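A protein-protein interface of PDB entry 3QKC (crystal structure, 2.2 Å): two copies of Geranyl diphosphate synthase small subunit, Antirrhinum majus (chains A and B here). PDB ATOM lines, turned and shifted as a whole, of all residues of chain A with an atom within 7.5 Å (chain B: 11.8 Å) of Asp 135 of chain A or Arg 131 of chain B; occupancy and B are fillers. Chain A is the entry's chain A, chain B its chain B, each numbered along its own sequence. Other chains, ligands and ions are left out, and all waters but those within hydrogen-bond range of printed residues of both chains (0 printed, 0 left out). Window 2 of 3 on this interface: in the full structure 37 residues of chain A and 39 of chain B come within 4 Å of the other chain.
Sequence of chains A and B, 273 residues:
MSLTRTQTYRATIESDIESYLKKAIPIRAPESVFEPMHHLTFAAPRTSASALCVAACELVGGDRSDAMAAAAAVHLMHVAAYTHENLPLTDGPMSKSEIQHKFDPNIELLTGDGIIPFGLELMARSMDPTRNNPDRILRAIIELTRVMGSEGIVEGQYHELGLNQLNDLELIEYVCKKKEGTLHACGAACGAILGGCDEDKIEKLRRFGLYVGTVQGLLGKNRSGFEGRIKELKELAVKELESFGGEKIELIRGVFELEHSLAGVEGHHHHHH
OD1 of Asp 135 of chain A is in salt-bridge range of NH1 of Arg 131 of chain B (3.4 Å).
OE2 of Glu 121 of chain B lies within salt-bridge range of NE of Arg 125 of chain B (3.0 Å). NE of Arg 131 of chain B lies within salt-bridge range of OD1 of Asp 128 of chain B, at 2.7 Å. The guanidinium group of Arg 139 of chain A lies within salt-bridge range of the side-chain carboxylate of Asp 135 of chain A (2.9 Å).
Leu 138 of chain B touches Met 127 of chain A (CD2 to CG, 3.4 Å). Pro 134 of chain A touches Leu 138 of chain B. CD1 of Leu 138 of chain B touches CG2 of Ile 137 of chain A, at 3.8 Å. Leu 138 of chain A touches Met 127 of chain B. O of Pro 134 of chain B touches CD2 of Leu 138 of chain A, at 3.9 Å. CD1 of Ile 141 of chain B touches CD1 of Leu 138 of chain A, at 3.5 Å. Ile 141 of chain A touches Ala 124 of chain B. Leu 138 of chain B touches Ile 141 of chain A. CB of Ala 124 of chain B touches CG1 of Ile 142 of chain A, at 3.8 Å. CG2 of Ile 142 of chain A touches NH1 of Arg 125 of chain B, at 3.8 Å.
Asp 135 of chain A touches just one residue of chain B: Arg 131 (3.4 Å). Ile 137 of chain A touches just one residue of chain B: Leu 138 (3.8 Å). Of chain B, only Met 127 (3.7 Å), Pro 134 (3.9 Å), Ile 137 (3.8 Å), Leu 138 (3.6 Å) and Ile 141 (3.5 Å) come within 4 Å of Leu 138 of chain A. No residue of chain B comes within 4 Å of Arg 139 of chain A. Of the printed residues of chain B, Ile 142 of chain A touches Ala 124 (3.8 Å) and Arg 125 (3.8 Å). Of the printed residues of chain A, Arg 125 of chain B touches Ile 142 (3.8 Å). Of chain A, only Asp 135 comes within 4 Å of Arg 131 of chain B. Of the printed residues of chain A, Leu 138 of chain B touches Met 127, Pro 134, Ile 137, Leu 138 and Ile 141. The nearest residue of chain A that does not touch Arg 131 of chain B is Arg 139 of chain A (6.9 Å).
Hydrophobic or aromatic side chains of chain A that line the printed part of chain B: Met 127, Pro 134, Ile 137, Leu 138, Ile 141 and Ile 142. Hydrophobic or aromatic side chains of chain B within 4 Å of the printed part of chain A: Ala 124, Met 127, Pro 134, Ile 137, Leu 138 and Ile 141. Among the printed residues, Asp or Glu carboxylates within 4 Å of a Lys or Arg side-chain nitrogen of the other chain: Asp 135 of chain A with Arg 131 of chain B (3.4 Å).
Met 127 of chain A touches Asp 135 of chain B, but with the chains exchanged Asp 135 of chain A does not touch Met 127 of chain B (4.6 Å). Pro 134 of chain B touches its own counterpart, Pro 134 of chain A. Pro 134 of chain A touches Leu 138 of chain B, and with the chains exchanged Leu 138 of chain A touches Pro 134 of chain B. Leu 138 of chain B touches its own counterpart, Leu 138 of chain A.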
ATOM      1  N   MET A 127     -28.439 -17.634  -2.574  1.00  0.00           N
ATOM      2  CA  MET A 127     -28.309 -18.729  -3.545  1.00  0.00           C
ATOM      3  C   MET A 127     -28.133 -20.079  -2.875  1.00  0.00           C
ATOM      4  O   MET A 127     -27.301 -20.224  -1.977  1.00  0.00           O
ATOM      5  CB  MET A 127     -27.143 -18.474  -4.507  1.00  0.00           C
ATOM      6  CG  MET A 127     -27.244 -19.222  -5.837  1.00  0.00           C
ATOM      7  SD  MET A 127     -26.590 -20.902  -5.830  1.00  0.00           S
ATOM      8  CE  MET A 127     -24.821 -20.595  -5.778  1.00  0.00           C
ATOM      9  N   ASN A 132     -30.869 -25.715  -7.040  1.00  0.00           N
ATOM     10  CA  ASN A 132     -31.073 -25.305  -8.452  1.00  0.00           C
ATOM     11  C   ASN A 132     -31.350 -23.795  -8.589  1.00  0.00           C
ATOM     12  O   ASN A 132     -31.732 -23.295  -9.665  1.00  0.00           O
ATOM     13  CB  ASN A 132     -32.175 -26.124  -9.149  1.00  0.00           C
ATOM     14  CG  ASN A 132     -33.585 -25.554  -8.938  1.00  0.00           C
ATOM     15  OD1 ASN A 132     -34.203 -25.743  -7.883  1.00  0.00           O
ATOM     16  ND2 ASN A 132     -34.106 -24.882  -9.964  1.00  0.00           N
ATOM     17  N   ASN A 133     -31.120 -23.086  -7.487  1.00  0.00           N
ATOM     18  CA  ASN A 133     -31.476 -21.675  -7.340  1.00  0.00           C
ATOM     19  C   ASN A 133     -30.854 -20.656  -8.306  1.00  0.00           C
ATOM     20  O   ASN A 133     -31.512 -19.679  -8.639  1.00  0.00           O
ATOM     21  CB  ASN A 133     -31.269 -21.234  -5.890  1.00  0.00           C
ATOM     22  CG  ASN A 133     -32.223 -21.926  -4.925  1.00  0.00           C
ATOM     23  OD1 ASN A 133     -32.601 -23.081  -5.128  1.00  0.00           O
ATOM     24  ND2 ASN A 133     -32.612 -21.223  -3.868  1.00  0.00           N
ATOM     25  N   PRO A 134     -29.601 -20.859  -8.764  1.00  0.00           N
ATOM     26  CA  PRO A 134     -29.041 -19.791  -9.607  1.00  0.00           C
ATOM     27  C   PRO A 134     -29.968 -19.365 -10.754  1.00  0.00           C
ATOM     28  O   PRO A 134     -30.075 -18.172 -11.041  1.00  0.00           O
ATOM     29  CB  PRO A 134     -27.738 -20.404 -10.145  1.00  0.00           C
ATOM     30  CG  PRO A 134     -27.880 -21.861  -9.937  1.00  0.00           C
ATOM     31  CD  PRO A 134     -28.681 -22.011  -8.690  1.00  0.00           C
ATOM     32  N   ASP A 135     -30.634 -20.331 -11.388  1.00  0.00           N
ATOM     33  CA  ASP A 135     -31.686 -20.048 -12.367  1.00  0.00           C
ATOM     34  C   ASP A 135     -32.867 -19.353 -11.685  1.00  0.00           C
ATOM     35  O   ASP A 135     -33.310 -18.302 -12.135  1.00  0.00           O
ATOM     36  CB  ASP A 135     -32.152 -21.341 -13.046  1.00  0.00           C
ATOM     37  CG  ASP A 135     -33.541 -21.216 -13.676  1.00  0.00           C
ATOM     38  OD1 ASP A 135     -33.685 -20.438 -14.649  1.00  0.00           O
ATOM     39  OD2 ASP A 135     -34.481 -21.909 -13.203  1.00  0.00           O
ATOM     40  N   ARG A 136     -33.348 -19.954 -10.597  1.00  0.00           N
ATOM     41  CA  ARG A 136     -34.497 -19.458  -9.831  1.00  0.00           C
ATOM     42  C   ARG A 136     -34.276 -18.097  -9.183  1.00  0.00           C
ATOM     43  O   ARG A 136     -35.083 -17.185  -9.362  1.00  0.00           O
ATOM     44  CB  ARG A 136     -34.859 -20.449  -8.730  1.00  0.00           C
ATOM     45  CG  ARG A 136     -36.012 -21.349  -9.065  1.00  0.00           C
ATOM     46  CD  ARG A 136     -36.242 -22.341  -7.958  1.00  0.00           C
ATOM     47  NE  ARG A 136     -36.943 -23.511  -8.465  1.00  0.00           N
ATOM     48  CZ  ARG A 136     -37.339 -24.539  -7.721  1.00  0.00           C
ATOM     49  NH1 ARG A 136     -37.117 -24.555  -6.411  1.00  0.00           N
ATOM     50  NH2 ARG A 136     -37.971 -25.547  -8.295  1.00  0.00           N
ATOM     51  N   ILE A 137     -33.205 -17.990  -8.396  1.00  0.00           N
ATOM     52  CA  ILE A 137     -32.873 -16.747  -7.687  1.00  0.00           C
ATOM     53  C   ILE A 137     -32.629 -15.610  -8.672  1.00  0.00           C
ATOM     54  O   ILE A 137     -33.073 -14.485  -8.446  1.00  0.00           O
ATOM     55  CB  ILE A 137     -31.710 -16.961  -6.682  1.00  0.00           C
ATOM     56  CG1 ILE A 137     -32.300 -17.443  -5.351  1.00  0.00           C
ATOM     57  CG2 ILE A 137     -30.887 -15.696  -6.484  1.00  0.00           C
ATOM     58  CD1 ILE A 137     -31.335 -18.142  -4.437  1.00  0.00           C
ATOM     59  N   LEU A 138     -31.982 -15.925  -9.786  1.00  0.00           N
ATOM     60  CA  LEU A 138     -31.768 -14.948 -10.847  1.00  0.00           C
ATOM     61  C   LEU A 138     -33.101 -14.507 -11.453  1.00  0.00           C
ATOM     62  O   LEU A 138     -33.283 -13.329 -11.767  1.00  0.00           O
ATOM     63  CB  LEU A 138     -30.848 -15.524 -11.920  1.00  0.00           C
ATOM     64  CG  LEU A 138     -29.926 -14.671 -12.789  1.00  0.00           C
ATOM     65  CD1 LEU A 138     -29.307 -13.511 -12.022  1.00  0.00           C
ATOM     66  CD2 LEU A 138     -28.836 -15.573 -13.386  1.00  0.00           C
ATOM     67  N   ARG A 139     -34.042 -15.444 -11.601  1.00  0.00           N
ATOM     68  CA  ARG A 139     -35.375 -15.086 -12.071  1.00  0.00           C
ATOM     69  C   ARG A 139     -36.127 -14.219 -11.062  1.00  0.00           C
ATOM     70  O   ARG A 139     -36.900 -13.354 -11.461  1.00  0.00           O
ATOM     71  CB  ARG A 139     -36.197 -16.318 -12.430  1.00  0.00           C
ATOM     72  CG  ARG A 139     -36.820 -16.253 -13.821  1.00  0.00           C
ATOM     73  CD  ARG A 139     -37.733 -17.450 -14.085  1.00  0.00           C
ATOM     74  NE  ARG A 139     -37.126 -18.724 -13.683  1.00  0.00           N
ATOM     75  CZ  ARG A 139     -37.821 -19.785 -13.272  1.00  0.00           C
ATOM     76  NH1 ARG A 139     -37.197 -20.913 -12.925  1.00  0.00           N
ATOM     77  NH2 ARG A 139     -39.145 -19.725 -13.213  1.00  0.00           N
ATOM     78  N   ALA A 140     -35.893 -14.448  -9.770  1.00  0.00           N
ATOM     79  CA  ALA A 140     -36.476 -13.615  -8.709  1.00  0.00           C
ATOM     80  C   ALA A 140     -35.938 -12.178  -8.741  1.00  0.00           C
ATOM     81  O   ALA A 140     -36.655 -11.221  -8.425  1.00  0.00           O
ATOM     82  CB  ALA A 140     -36.225 -14.241  -7.332  1.00  0.00           C
ATOM     83  N   ILE A 141     -34.671 -12.045  -9.114  1.00  0.00           N
ATOM     84  CA  ILE A 141     -34.001 -10.753  -9.193  1.00  0.00           C
ATOM     85  C   ILE A 141     -34.580  -9.956 -10.355  1.00  0.00           C
ATOM     86  O   ILE A 141     -34.841  -8.769 -10.224  1.00  0.00           O
ATOM     87  CB  ILE A 141     -32.468 -10.916  -9.317  1.00  0.00           C
ATOM     88  CG1 ILE A 141     -31.832 -10.921  -7.931  1.00  0.00           C
ATOM     89  CG2 ILE A 141     -31.843  -9.799 -10.148  1.00  0.00           C
ATOM     90  CD1 ILE A 141     -31.245 -12.243  -7.519  1.00  0.00           C
ATOM     91  N   ILE A 142     -34.830 -10.634 -11.470  1.00  0.00           N
ATOM     92  CA  ILE A 142     -35.493 -10.015 -12.604  1.00  0.00           C
ATOM     93  C   ILE A 142     -36.823  -9.400 -12.171  1.00  0.00           C
ATOM     94  O   ILE A 142     -37.099  -8.233 -12.500  1.00  0.00           O
ATOM     95  CB  ILE A 142     -35.674 -11.011 -13.765  1.00  0.00           C
ATOM     96  CG1 ILE A 142     -34.331 -11.225 -14.467  1.00  0.00           C
ATOM     97  CG2 ILE A 142     -36.713 -10.508 -14.756  1.00  0.00           C
ATOM     98  CD1 ILE A 142     -34.037 -12.680 -14.831  1.00  0.00           C
ATOM     99  N   ILE A 193     -41.952 -18.481  -8.049  1.00  0.00           N
ATOM    100  CA  ILE A 193     -40.650 -18.872  -8.596  1.00  0.00           C
ATOM    101  C   ILE A 193     -39.853 -19.642  -7.550  1.00  0.00           C
ATOM    102  O   ILE A 193     -39.313 -20.711  -7.837  1.00  0.00           O
ATOM    103  CB  ILE A 193     -39.818 -17.648  -9.107  1.00  0.00           C
ATOM    104  CG1 ILE A 193     -40.445 -17.023 -10.362  1.00  0.00           C
ATOM    105  CG2 ILE A 193     -38.349 -18.049  -9.406  1.00  0.00           C
ATOM    106  CD1 ILE A 193     -39.857 -15.644 -10.720  1.00  0.00           C
ATOM    107  N   ASP B  66     -19.293 -10.669 -23.411  1.00  0.00           N
ATOM    108  CA  ASP B  66     -19.462 -11.296 -22.093  1.00  0.00           C
ATOM    109  C   ASP B  66     -19.570 -10.279 -20.945  1.00  0.00           C
ATOM    110  O   ASP B  66     -20.150 -10.592 -19.897  1.00  0.00           O
ATOM    111  CB  ASP B  66     -18.296 -12.242 -21.794  1.00  0.00           C
ATOM    112  CG  ASP B  66     -18.394 -13.571 -22.533  1.00  0.00           C
ATOM    113  OD1 ASP B  66     -17.333 -14.223 -22.699  1.00  0.00           O
ATOM    114  OD2 ASP B  66     -19.518 -13.971 -22.920  1.00  0.00           O
ATOM    115  N   GLU B 121     -31.112  -5.300 -13.917  1.00  0.00           N
ATOM    116  CA  GLU B 121     -32.012  -6.059 -14.801  1.00  0.00           C
ATOM    117  C   GLU B 121     -31.316  -6.438 -16.119  1.00  0.00           C
ATOM    118  O   GLU B 121     -31.419  -7.583 -16.554  1.00  0.00           O
ATOM    119  CB  GLU B 121     -33.295  -5.277 -15.092  1.00  0.00           C
ATOM    120  CG  GLU B 121     -34.330  -6.064 -15.895  1.00  0.00           C
ATOM    121  CD  GLU B 121     -35.547  -5.248 -16.315  1.00  0.00           C
ATOM    122  OE1 GLU B 121     -35.796  -4.152 -15.759  1.00  0.00           O
ATOM    123  OE2 GLU B 121     -36.270  -5.706 -17.219  1.00  0.00           O
ATOM    124  N   MET B 123     -28.084  -6.775 -16.625  1.00  0.00           N
ATOM    125  CA  MET B 123     -27.104  -7.762 -16.186  1.00  0.00           C
ATOM    126  C   MET B 123     -27.755  -9.118 -15.900  1.00  0.00           C
ATOM    127  O   MET B 123     -27.254 -10.153 -16.348  1.00  0.00           O
ATOM    128  CB  MET B 123     -26.324  -7.228 -14.966  1.00  0.00           C
ATOM    129  CG  MET B 123     -25.267  -8.154 -14.392  1.00  0.00           C
ATOM    130  SD  MET B 123     -23.686  -8.201 -15.276  1.00  0.00           S
ATOM    131  CE  MET B 123     -24.009  -9.415 -16.534  1.00  0.00           C
ATOM    132  N   ALA B 124     -28.875  -9.102 -15.171  1.00  0.00           N
ATOM    133  CA  ALA B 124     -29.643 -10.320 -14.876  1.00  0.00           C
ATOM    134  C   ALA B 124     -30.224 -11.001 -16.121  1.00  0.00           C
ATOM    135  O   ALA B 124     -30.319 -12.225 -16.165  1.00  0.00           O
ATOM    136  CB  ALA B 124     -30.748 -10.033 -13.867  1.00  0.00           C
ATOM    137  N   ARG B 125     -30.605 -10.210 -17.121  1.00  0.00           N
ATOM    138  CA  ARG B 125     -31.271 -10.735 -18.323  1.00  0.00           C
ATOM    139  C   ARG B 125     -30.307 -11.096 -19.456  1.00  0.00           C
ATOM    140  O   ARG B 125     -30.739 -11.576 -20.506  1.00  0.00           O
ATOM    141  CB  ARG B 125     -32.295  -9.733 -18.861  1.00  0.00           C
ATOM    142  CG  ARG B 125     -33.620  -9.639 -18.117  1.00  0.00           C
ATOM    143  CD  ARG B 125     -34.625  -8.943 -19.031  1.00  0.00           C
ATOM    144  NE  ARG B 125     -35.823  -8.409 -18.384  1.00  0.00           N
ATOM    145  CZ  ARG B 125     -36.968  -9.077 -18.247  1.00  0.00           C
ATOM    146  NH1 ARG B 125     -38.011  -8.494 -17.674  1.00  0.00           N
ATOM    147  NH2 ARG B 125     -37.078 -10.328 -18.670  1.00  0.00           N
ATOM    148  N   SER B 126     -29.013 -10.851 -19.256  1.00  0.00           N
ATOM    149  CA  SER B 126     -28.015 -11.196 -20.265  1.00  0.00           C
ATOM    150  C   SER B 126     -27.787 -12.714 -20.331  1.00  0.00           C
ATOM    151  O   SER B 126     -27.742 -13.290 -21.427  1.00  0.00           O
ATOM    152  CB  SER B 126     -26.706 -10.412 -20.063  1.00  0.00           C
ATOM    153  OG  SER B 126     -26.038 -10.770 -18.866  1.00  0.00           O
ATOM    154  N   MET B 127     -27.690 -13.357 -19.163  1.00  0.00           N
ATOM    155  CA  MET B 127     -27.551 -14.822 -19.061  1.00  0.00           C
ATOM    156  C   MET B 127     -28.692 -15.550 -19.759  1.00  0.00           C
ATOM    157  O   MET B 127     -29.740 -14.955 -20.034  1.00  0.00           O
ATOM    158  CB  MET B 127     -27.469 -15.264 -17.585  1.00  0.00           C
ATOM    159  CG  MET B 127     -28.622 -16.133 -17.041  1.00  0.00           C
ATOM    160  SD  MET B 127     -28.310 -17.927 -17.090  1.00  0.00           S
ATOM    161  CE  MET B 127     -29.909 -18.557 -16.578  1.00  0.00           C
ATOM    162  N   ASP B 128     -28.471 -16.831 -20.061  1.00  0.00           N
ATOM    163  CA  ASP B 128     -29.551 -17.746 -20.452  1.00  0.00           C
ATOM    164  C   ASP B 128     -29.654 -18.108 -21.950  1.00  0.00           C
ATOM    165  O   ASP B 128     -30.170 -19.191 -22.264  1.00  0.00           O
ATOM    166  CB  ASP B 128     -30.904 -17.233 -19.898  1.00  0.00           C
ATOM    167  CG  ASP B 128     -32.069 -18.141 -20.226  1.00  0.00           C
ATOM    168  OD1 ASP B 128     -31.988 -19.351 -19.945  1.00  0.00           O
ATOM    169  OD2 ASP B 128     -33.078 -17.628 -20.754  1.00  0.00           O
ATOM    170  N   PRO B 129     -29.152 -17.246 -22.875  1.00  0.00           N
ATOM    171  CA  PRO B 129     -29.402 -17.552 -24.290  1.00  0.00           C
ATOM    172  C   PRO B 129     -29.169 -19.029 -24.627  1.00  0.00           C
ATOM    173  O   PRO B 129     -30.063 -19.675 -25.175  1.00  0.00           O
ATOM    174  CB  PRO B 129     -28.403 -16.653 -25.028  1.00  0.00           C
ATOM    175  CG  PRO B 129     -28.226 -15.494 -24.121  1.00  0.00           C
ATOM    176  CD  PRO B 129     -28.242 -16.091 -22.740  1.00  0.00           C
ATOM    177  N   THR B 130     -27.991 -19.547 -24.281  1.00  0.00           N
ATOM    178  CA  THR B 130     -27.685 -20.979 -24.414  1.00  0.00           C
ATOM    179  C   THR B 130     -27.441 -21.630 -23.036  1.00  0.00           C
ATOM    180  O   THR B 130     -26.943 -22.762 -22.949  1.00  0.00           O
ATOM    181  CB  THR B 130     -26.503 -21.238 -25.404  1.00  0.00           C
ATOM    182  OG1 THR B 130     -26.321 -22.649 -25.588  1.00  0.00           O
ATOM    183  CG2 THR B 130     -25.195 -20.602 -24.910  1.00  0.00           C
ATOM    184  N   ARG B 131     -27.837 -20.904 -21.981  1.00  0.00           N
ATOM    185  CA  ARG B 131     -27.635 -21.269 -20.564  1.00  0.00           C
ATOM    186  C   ARG B 131     -26.212 -20.937 -20.101  1.00  0.00           C
ATOM    187  O   ARG B 131     -25.352 -21.822 -19.985  1.00  0.00           O
ATOM    188  CB  ARG B 131     -27.998 -22.739 -20.262  1.00  0.00           C
ATOM    189  CG  ARG B 131     -29.391 -23.226 -20.733  1.00  0.00           C
ATOM    190  CD  ARG B 131     -30.472 -22.141 -20.713  1.00  0.00           C
ATOM    191  NE  ARG B 131     -30.773 -21.662 -19.364  1.00  0.00           N
ATOM    192  CZ  ARG B 131     -31.916 -21.891 -18.726  1.00  0.00           C
ATOM    193  NH1 ARG B 131     -32.093 -21.414 -17.503  1.00  0.00           N
ATOM    194  NH2 ARG B 131     -32.888 -22.583 -19.311  1.00  0.00           N
ATOM    195  N   ASN B 132     -25.983 -19.649 -19.841  1.00  0.00           N
ATOM    196  CA  ASN B 132     -24.653 -19.135 -19.514  1.00  0.00           C
ATOM    197  C   ASN B 132     -24.501 -18.558 -18.107  1.00  0.00           C
ATOM    198  O   ASN B 132     -25.143 -17.556 -17.749  1.00  0.00           O
ATOM    199  CB  ASN B 132     -24.222 -18.054 -20.513  1.00  0.00           C
ATOM    200  CG  ASN B 132     -24.073 -18.572 -21.917  1.00  0.00           C
ATOM    201  OD1 ASN B 132     -24.524 -17.930 -22.863  1.00  0.00           O
ATOM    202  ND2 ASN B 132     -23.429 -19.729 -22.072  1.00  0.00           N
ATOM    203  N   ASN B 133     -23.620 -19.187 -17.329  1.00  0.00           N
ATOM    204  CA  ASN B 133     -23.073 -18.600 -16.099  1.00  0.00           C
ATOM    205  C   ASN B 133     -24.099 -18.037 -15.096  1.00  0.00           C
ATOM    206  O   ASN B 133     -24.110 -16.833 -14.847  1.00  0.00           O
ATOM    207  CB  ASN B 133     -22.070 -17.491 -16.452  1.00  0.00           C
ATOM    208  CG  ASN B 133     -21.599 -17.549 -17.895  1.00  0.00           C
ATOM    209  OD1 ASN B 133     -20.929 -18.498 -18.312  1.00  0.00           O
ATOM    210  ND2 ASN B 133     -21.940 -16.514 -18.664  1.00  0.00           N
ATOM    211  N   PRO B 134     -24.956 -18.896 -14.512  1.00  0.00           N
ATOM    212  CA  PRO B 134     -25.939 -18.378 -13.559  1.00  0.00           C
ATOM    213  C   PRO B 134     -25.321 -18.007 -12.217  1.00  0.00           C
ATOM    214  O   PRO B 134     -25.745 -17.033 -11.595  1.00  0.00           O
ATOM    215  CB  PRO B 134     -26.915 -19.550 -13.375  1.00  0.00           C
ATOM    216  CG  PRO B 134     -26.603 -20.500 -14.456  1.00  0.00           C
ATOM    217  CD  PRO B 134     -25.159 -20.332 -14.762  1.00  0.00           C
ATOM    218  N   ASP B 135     -24.342 -18.790 -11.770  1.00  0.00           N
ATOM    219  CA  ASP B 135     -23.599 -18.458 -10.561  1.00  0.00           C
ATOM    220  C   ASP B 135     -22.679 -17.261 -10.805  1.00  0.00           C
ATOM    221  O   ASP B 135     -22.472 -16.446  -9.908  1.00  0.00           O
ATOM    222  CB  ASP B 135     -22.789 -19.655 -10.066  1.00  0.00           C
ATOM    223  CG  ASP B 135     -22.023 -19.351  -8.794  1.00  0.00           C
ATOM    224  OD1 ASP B 135     -22.672 -19.101  -7.759  1.00  0.00           O
ATOM    225  OD2 ASP B 135     -20.775 -19.353  -8.832  1.00  0.00           O
ATOM    226  N   ARG B 136     -22.138 -17.162 -12.019  1.00  0.00           N
ATOM    227  CA  ARG B 136     -21.305 -16.022 -12.406  1.00  0.00           C
ATOM    228  C   ARG B 136     -22.099 -14.725 -12.493  1.00  0.00           C
ATOM    229  O   ARG B 136     -21.693 -13.717 -11.918  1.00  0.00           O
ATOM    230  CB  ARG B 136     -20.615 -16.261 -13.744  1.00  0.00           C
ATOM    231  CG  ARG B 136     -19.234 -16.854 -13.652  1.00  0.00           C
ATOM    232  CD  ARG B 136     -18.671 -17.041 -15.044  1.00  0.00           C
ATOM    233  NE  ARG B 136     -17.677 -18.108 -15.082  1.00  0.00           N
ATOM    234  CZ  ARG B 136     -16.980 -18.453 -16.160  1.00  0.00           C
ATOM    235  NH1 ARG B 136     -17.144 -17.809 -17.312  1.00  0.00           N
ATOM    236  NH2 ARG B 136     -16.102 -19.440 -16.077  1.00  0.00           N
ATOM    237  N   ILE B 137     -23.214 -14.745 -13.224  1.00  0.00           N
ATOM    238  CA  ILE B 137     -24.004 -13.525 -13.405  1.00  0.00           C
ATOM    239  C   ILE B 137     -24.594 -13.084 -12.075  1.00  0.00           C
ATOM    240  O   ILE B 137     -24.673 -11.893 -11.791  1.00  0.00           O
ATOM    241  CB  ILE B 137     -25.031 -13.643 -14.566  1.00  0.00           C
ATOM    242  CG1 ILE B 137     -24.387 -13.068 -15.834  1.00  0.00           C
ATOM    243  CG2 ILE B 137     -26.311 -12.869 -14.264  1.00  0.00           C
ATOM    244  CD1 ILE B 137     -24.744 -13.772 -17.126  1.00  0.00           C
ATOM    245  N   LEU B 138     -24.947 -14.060 -11.245  1.00  0.00           N
ATOM    246  CA  LEU B 138     -25.367 -13.795  -9.882  1.00  0.00           C
ATOM    247  C   LEU B 138     -24.230 -13.157  -9.092  1.00  0.00           C
ATOM    248  O   LEU B 138     -24.454 -12.200  -8.349  1.00  0.00           O
ATOM    249  CB  LEU B 138     -25.803 -15.090  -9.210  1.00  0.00           C
ATOM    250  CG  LEU B 138     -26.958 -15.128  -8.219  1.00  0.00           C
ATOM    251  CD1 LEU B 138     -28.118 -14.266  -8.692  1.00  0.00           C
ATOM    252  CD2 LEU B 138     -27.400 -16.598  -8.053  1.00  0.00           C
ATOM    253  N   ARG B 139     -23.012 -13.679  -9.250  1.00  0.00           N
ATOM    254  CA  ARG B 139     -21.874 -13.079  -8.566  1.00  0.00           C
ATOM    255  C   ARG B 139     -21.569 -11.658  -9.050  1.00  0.00           C
ATOM    256  O   ARG B 139     -21.170 -10.812  -8.250  1.00  0.00           O
ATOM    257  CB  ARG B 139     -20.617 -13.954  -8.634  1.00  0.00           C
ATOM    258  CG  ARG B 139     -19.521 -13.467  -7.675  1.00  0.00           C
ATOM    259  CD  ARG B 139     -18.394 -14.468  -7.528  1.00  0.00           C
ATOM    260  NE  ARG B 139     -17.245 -13.914  -6.810  1.00  0.00           N
ATOM    261  CZ  ARG B 139     -16.103 -14.575  -6.611  1.00  0.00           C
ATOM    262  NH1 ARG B 139     -15.952 -15.810  -7.086  1.00  0.00           N
ATOM    263  NH2 ARG B 139     -15.105 -14.009  -5.938  1.00  0.00           N
ATOM    264  N   ILE B 141     -23.778  -9.612 -10.095  1.00  0.00           N
ATOM    265  CA  ILE B 141     -24.879  -8.834  -9.547  1.00  0.00           C
ATOM    266  C   ILE B 141     -24.574  -8.438  -8.108  1.00  0.00           C
ATOM    267  O   ILE B 141     -24.772  -7.280  -7.711  1.00  0.00           O
ATOM    268  CB  ILE B 141     -26.192  -9.613  -9.691  1.00  0.00           C
ATOM    269  CG1 ILE B 141     -26.755  -9.355 -11.089  1.00  0.00           C
ATOM    270  CG2 ILE B 141     -27.199  -9.258  -8.591  1.00  0.00           C
ATOM    271  CD1 ILE B 141     -27.608 -10.465 -11.609  1.00  0.00           C
ATOM    272  N   LEU B 194     -16.816 -12.435 -15.065  1.00  0.00           N
ATOM    273  CA  LEU B 194     -17.440 -12.779 -16.340  1.00  0.00           C
ATOM    274  C   LEU B 194     -16.413 -13.362 -17.279  1.00  0.00           C
ATOM    275  O   LEU B 194     -16.739 -14.166 -18.145  1.00  0.00           O
ATOM    276  CB  LEU B 194     -18.164 -11.566 -16.945  1.00  0.00           C
ATOM    277  CG  LEU B 194     -19.315 -11.133 -16.009  1.00  0.00           C
ATOM    278  CD1 LEU B 194     -19.754  -9.669 -16.222  1.00  0.00           C
ATOM    279  CD2 LEU B 194     -20.508 -12.091 -16.126  1.00  0.00           C
